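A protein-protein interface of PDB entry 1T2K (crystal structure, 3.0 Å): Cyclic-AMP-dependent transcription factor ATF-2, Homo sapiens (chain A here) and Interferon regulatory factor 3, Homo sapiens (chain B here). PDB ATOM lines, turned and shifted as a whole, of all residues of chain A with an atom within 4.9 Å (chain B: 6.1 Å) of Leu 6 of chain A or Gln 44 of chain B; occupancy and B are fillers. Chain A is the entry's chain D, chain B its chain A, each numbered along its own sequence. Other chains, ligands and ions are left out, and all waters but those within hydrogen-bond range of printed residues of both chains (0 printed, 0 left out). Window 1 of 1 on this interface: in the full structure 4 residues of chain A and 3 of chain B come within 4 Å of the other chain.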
ATOM      1  N   ARG A   2      -2.744  21.829  -2.938  1.00  0.00           N
ATOM      2  CA  ARG A   2      -2.977  21.354  -1.581  1.00  0.00           C
ATOM      3  C   ARG A   2      -3.724  22.342  -0.693  1.00  0.00           C
ATOM      4  O   ARG A   2      -4.629  21.960   0.043  1.00  0.00           O
ATOM      5  CB  ARG A   2      -1.665  21.044  -0.874  1.00  0.00           C
ATOM      6  CG  ARG A   2      -1.904  20.640   0.553  1.00  0.00           C
ATOM      7  CD  ARG A   2      -2.875  19.494   0.527  1.00  0.00           C
ATOM      8  NE  ARG A   2      -3.351  19.101   1.839  1.00  0.00           N
ATOM      9  CZ  ARG A   2      -2.565  18.828   2.875  1.00  0.00           C
ATOM     10  NH1 ARG A   2      -1.244  18.915   2.753  1.00  0.00           N
ATOM     11  NH2 ARG A   2      -3.108  18.442   4.032  1.00  0.00           N
ATOM     12  N   ARG A   3      -3.369  23.618  -0.796  1.00  0.00           N
ATOM     13  CA  ARG A   3      -3.970  24.627   0.058  1.00  0.00           C
ATOM     14  C   ARG A   3      -5.448  24.865  -0.179  1.00  0.00           C
ATOM     15  O   ARG A   3      -6.208  25.020   0.785  1.00  0.00           O
ATOM     16  CB  ARG A   3      -3.208  25.949  -0.065  1.00  0.00           C
ATOM     17  CG  ARG A   3      -1.831  26.004   0.655  1.00  0.00           C
ATOM     18  CD  ARG A   3      -1.922  26.043   2.204  1.00  0.00           C
ATOM     19  NE  ARG A   3      -1.831  24.717   2.832  1.00  0.00           N
ATOM     20  CZ  ARG A   3      -0.690  24.088   3.135  1.00  0.00           C
ATOM     21  NH1 ARG A   3       0.481  24.660   2.875  1.00  0.00           N
ATOM     22  NH2 ARG A   3      -0.717  22.880   3.701  1.00  0.00           N
ATOM     23  N   LYS A   4      -5.874  24.900  -1.439  1.00  0.00           N
ATOM     24  CA  LYS A   4      -7.291  25.090  -1.724  1.00  0.00           C
ATOM     25  C   LYS A   4      -8.120  23.920  -1.287  1.00  0.00           C
ATOM     26  O   LYS A   4      -9.248  24.101  -0.852  1.00  0.00           O
ATOM     27  CB  LYS A   4      -7.578  25.476  -3.162  1.00  0.00           C
ATOM     28  CG  LYS A   4      -7.837  26.964  -3.218  1.00  0.00           C
ATOM     29  CD  LYS A   4      -8.250  27.439  -4.573  1.00  0.00           C
ATOM     30  CE  LYS A   4      -9.660  27.028  -4.892  1.00  0.00           C
ATOM     31  NZ  LYS A   4     -10.033  27.575  -6.224  1.00  0.00           N
ATOM     32  N   PHE A   5      -7.591  22.707  -1.421  1.00  0.00           N
ATOM     33  CA  PHE A   5      -8.381  21.554  -0.998  1.00  0.00           C
ATOM     34  C   PHE A   5      -8.635  21.661   0.510  1.00  0.00           C
ATOM     35  O   PHE A   5      -9.749  21.383   0.973  1.00  0.00           O
ATOM     36  CB  PHE A   5      -7.621  20.257  -1.278  1.00  0.00           C
ATOM     37  CG  PHE A   5      -8.055  19.100  -0.420  1.00  0.00           C
ATOM     38  CD1 PHE A   5      -9.323  18.555  -0.554  1.00  0.00           C
ATOM     39  CD2 PHE A   5      -7.190  18.555   0.528  1.00  0.00           C
ATOM     40  CE1 PHE A   5      -9.726  17.476   0.243  1.00  0.00           C
ATOM     41  CE2 PHE A   5      -7.584  17.475   1.333  1.00  0.00           C
ATOM     42  CZ  PHE A   5      -8.852  16.936   1.189  1.00  0.00           C
ATOM     43  N   LEU A   6      -7.622  22.067   1.276  1.00  0.00           N
ATOM     44  CA  LEU A   6      -7.801  22.224   2.710  1.00  0.00           C
ATOM     45  C   LEU A   6      -8.739  23.362   3.067  1.00  0.00           C
ATOM     46  O   LEU A   6      -9.592  23.230   3.945  1.00  0.00           O
ATOM     47  CB  LEU A   6      -6.460  22.443   3.374  1.00  0.00           C
ATOM     48  CG  LEU A   6      -5.679  21.152   3.535  1.00  0.00           C
ATOM     49  CD1 LEU A   6      -4.313  21.496   4.101  1.00  0.00           C
ATOM     50  CD2 LEU A   6      -6.433  20.175   4.452  1.00  0.00           C
ATOM     51  N   GLU A   7      -8.601  24.471   2.359  1.00  0.00           N
ATOM     52  CA  GLU A   7      -9.436  25.630   2.609  1.00  0.00           C
ATOM     53  C   GLU A   7     -10.879  25.270   2.310  1.00  0.00           C
ATOM     54  O   GLU A   7     -11.797  25.688   3.000  1.00  0.00           O
ATOM     55  CB  GLU A   7      -8.994  26.782   1.724  1.00  0.00           C
ATOM     56  CG  GLU A   7     -10.123  27.645   1.232  1.00  0.00           C
ATOM     57  CD  GLU A   7      -9.611  28.872   0.493  1.00  0.00           C
ATOM     58  OE1 GLU A   7      -8.723  28.712  -0.387  1.00  0.00           O
ATOM     59  OE2 GLU A   7     -10.096  29.993   0.792  1.00  0.00           O
ATOM     60  N   ARG A   8     -11.080  24.509   1.250  1.00  0.00           N
ATOM     61  CA  ARG A   8     -12.419  24.079   0.893  1.00  0.00           C
ATOM     62  C   ARG A   8     -13.054  23.101   1.903  1.00  0.00           C
ATOM     63  O   ARG A   8     -14.210  23.275   2.297  1.00  0.00           O
ATOM     64  CB  ARG A   8     -12.358  23.391  -0.477  1.00  0.00           C
ATOM     65  CG  ARG A   8     -13.016  24.153  -1.616  1.00  0.00           C
ATOM     66  CD  ARG A   8     -12.947  23.383  -2.940  1.00  0.00           C
ATOM     67  NE  ARG A   8     -13.954  23.860  -3.887  1.00  0.00           N
ATOM     68  CZ  ARG A   8     -14.148  25.143  -4.210  1.00  0.00           C
ATOM     69  NH1 ARG A   8     -13.403  26.105  -3.670  1.00  0.00           N
ATOM     70  NH2 ARG A   8     -15.102  25.472  -5.074  1.00  0.00           N
ATOM     71  N   ASN A   9     -12.275  22.137   2.390  1.00  0.00           N
ATOM     72  CA  ASN A   9     -12.829  21.131   3.285  1.00  0.00           C
ATOM     73  C   ASN A   9     -13.290  21.803   4.552  1.00  0.00           C
ATOM     74  O   ASN A   9     -14.379  21.541   5.076  1.00  0.00           O
ATOM     75  CB  ASN A   9     -11.758  20.075   3.619  1.00  0.00           C
ATOM     76  CG  ASN A   9     -12.274  18.968   4.550  1.00  0.00           C
ATOM     77  OD1 ASN A   9     -11.496  18.231   5.193  1.00  0.00           O
ATOM     78  ND2 ASN A   9     -13.589  18.842   4.617  1.00  0.00           N
ATOM     79  N   ARG A  10     -12.459  22.733   4.997  1.00  0.00           N
ATOM     80  CA  ARG A  10     -12.706  23.441   6.222  1.00  0.00           C
ATOM     81  C   ARG A  10     -13.947  24.307   6.142  1.00  0.00           C
ATOM     82  O   ARG A  10     -14.738  24.331   7.084  1.00  0.00           O
ATOM     83  CB  ARG A  10     -11.448  24.241   6.565  1.00  0.00           C
ATOM     84  CG  ARG A  10     -11.659  25.607   7.171  1.00  0.00           C
ATOM     85  CD  ARG A  10     -10.700  26.607   6.498  1.00  0.00           C
ATOM     86  NE  ARG A  10      -9.311  26.143   6.554  1.00  0.00           N
ATOM     87  CZ  ARG A  10      -8.314  26.660   5.844  1.00  0.00           C
ATOM     88  NH1 ARG A  10      -8.536  27.666   5.005  1.00  0.00           N
ATOM     89  NH2 ARG A  10      -7.091  26.162   6.000  1.00  0.00           N
ATOM     90  N   LEU B  42      -4.259  25.988  14.032  1.00  0.00           N
ATOM     91  CA  LEU B  42      -4.368  24.621  13.528  1.00  0.00           C
ATOM     92  C   LEU B  42      -4.196  24.619  12.024  1.00  0.00           C
ATOM     93  O   LEU B  42      -3.955  23.572  11.421  1.00  0.00           O
ATOM     94  CB  LEU B  42      -5.717  23.988  13.895  1.00  0.00           C
ATOM     95  CG  LEU B  42      -5.702  23.145  15.168  1.00  0.00           C
ATOM     96  CD1 LEU B  42      -7.064  22.514  15.422  1.00  0.00           C
ATOM     97  CD2 LEU B  42      -4.645  22.079  15.011  1.00  0.00           C
ATOM     98  N   ARG B  43      -4.332  25.786  11.404  1.00  0.00           N
ATOM     99  CA  ARG B  43      -4.143  25.836   9.968  1.00  0.00           C
ATOM    100  C   ARG B  43      -2.685  25.477   9.758  1.00  0.00           C
ATOM    101  O   ARG B  43      -1.819  26.066  10.390  1.00  0.00           O
ATOM    102  CB  ARG B  43      -4.443  27.235   9.419  1.00  0.00           C
ATOM    103  CG  ARG B  43      -5.924  27.541   9.385  1.00  0.00           C
ATOM    104  CD  ARG B  43      -6.233  28.929   8.855  1.00  0.00           C
ATOM    105  NE  ARG B  43      -6.060  29.080   7.413  1.00  0.00           N
ATOM    106  CZ  ARG B  43      -6.453  30.163   6.748  1.00  0.00           C
ATOM    107  NH1 ARG B  43      -7.034  31.170   7.396  1.00  0.00           N
ATOM    108  NH2 ARG B  43      -6.270  30.251   5.440  1.00  0.00           N
ATOM    109  N   GLN B  44      -2.411  24.488   8.911  1.00  0.00           N
ATOM    110  CA  GLN B  44      -1.029  24.100   8.650  1.00  0.00           C
ATOM    111  C   GLN B  44      -0.268  25.291   8.077  1.00  0.00           C
ATOM    112  O   GLN B  44       0.901  25.505   8.388  1.00  0.00           O
ATOM    113  CB  GLN B  44      -0.982  22.924   7.670  1.00  0.00           C
ATOM    114  CG  GLN B  44      -1.184  21.564   8.332  1.00  0.00           C
ATOM    115  CD  GLN B  44      -1.338  20.432   7.319  1.00  0.00           C
ATOM    116  OE1 GLN B  44      -1.309  20.658   6.106  1.00  0.00           O
ATOM    117  NE2 GLN B  44      -1.494  19.203   7.817  1.00  0.00           N
ATOM    118  N   ASP B  45      -0.941  26.059   7.228  1.00  0.00           N
ATOM    119  CA  ASP B  45      -0.332  27.237   6.629  1.00  0.00           C
ATOM    120  C   ASP B  45      -0.358  28.305   7.718  1.00  0.00           C
ATOM    121  O   ASP B  45      -1.146  29.238   7.665  1.00  0.00           O
ATOM    122  CB  ASP B  45      -1.142  27.702   5.405  1.00  0.00           C
ATOM    123  CG  ASP B  45      -2.575  28.088   5.746  1.00  0.00           C
ATOM    124  OD1 ASP B  45      -3.292  27.261   6.354  1.00  0.00           O
ATOM    125  OD2 ASP B  45      -2.998  29.211   5.383  1.00  0.00           O
ATOM    126  N   ALA B  46       0.508  28.148   8.685  1.00  0.00           N
ATOM    127  CA  ALA B  46       0.616  29.173   9.708  1.00  0.00           C
ATOM    128  C   ALA B  46       2.068  29.435   9.939  1.00  0.00           C
ATOM    129  O   ALA B  46       2.866  28.532  10.199  1.00  0.00           O
ATOM    130  CB  ALA B  46      -0.069  28.744  11.005  1.00  0.00           C
ATOM    131  N   GLN B  47       2.407  30.685   9.816  1.00  0.00           N
ATOM    132  CA  GLN B  47       3.728  31.138  10.107  1.00  0.00           C
ATOM    133  C   GLN B  47       3.642  32.002  11.352  1.00  0.00           C
ATOM    134  O   GLN B  47       2.585  32.553  11.671  1.00  0.00           O
ATOM    135  CB  GLN B  47       4.335  31.910   8.941  1.00  0.00           C
ATOM    136  CG  GLN B  47       3.353  32.894   8.329  1.00  0.00           C
ATOM    137  CD  GLN B  47       3.880  33.580   7.074  1.00  0.00           C
ATOM    138  OE1 GLN B  47       4.767  34.437   7.150  1.00  0.00           O
ATOM    139  NE2 GLN B  47       3.478  33.368   5.842  1.00  0.00           N
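NH2 of Arg 43 of chain B is in salt-bridge range of OD2 of Asp 45 of chain B (3.4 Å).
Of the printed residues of chain B, Arg 2 of chain A touches Gln 44 (3.5 Å).
Of the printed residues of chain B, Leu 6 of chain A touches Gln 44.
Asn 9 of chain A touches none of the printed residues of chain B.
Printed residues of chain B within 4 Å of Arg 10 of chain A: Arg 43 and Asp 45.
Of the printed residues of chain A, Arg 43 of chain B touches Arg 10 (3.4 Å).
Of chain A, only Arg 2, Arg 3 and Leu 6 come within 4 Å of Gln 44 of chain B.
Printed residues of chain A within 4 Å of Asp 45 of chain B: Arg 3 (3.7 Å) and Arg 10 (3.97 Å).
Among the printed residues, pairs that only touch across the chains: Arg 2 of chain A with Gln 44 of chain B (3.5 Å), Arg 3 of chain A with Asp 45 of chain B (3.7 Å) and Leu 6 of chain A with Gln 44 of chain B (3.7 Å).
OE1 of Gln 44 of chain B sits at hydrogen-bond distance from NH2 of Arg 3 of chain A, 3.3 Å away.
The side-chain carboxylate of Asp 45 of chain B lies within salt-bridge range of the guanidinium group of Arg 10 of chain A (3.97 Å).
The guanidinium group (NE) of Arg 43 of chain B sits close to the guanidinium group (NH2) of Arg 10 of chain A (3.4 Å).
Of the 9 printed residues of chain A, 4 touch a printed residue of chain B.
Of the 6 printed residues of chain B, 3 touch a printed residue of chain A.
Printed residues of chain B that touch a printed residue of chain A: Arg 43, Gln 44 and Asp 45.
Among the printed residues, Asp or Glu carboxylates within 4 Å of a Lys or Arg side-chain nitrogen of the other chain: Arg 10 of chain A with Asp 45 of chain B (3.97 Å).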
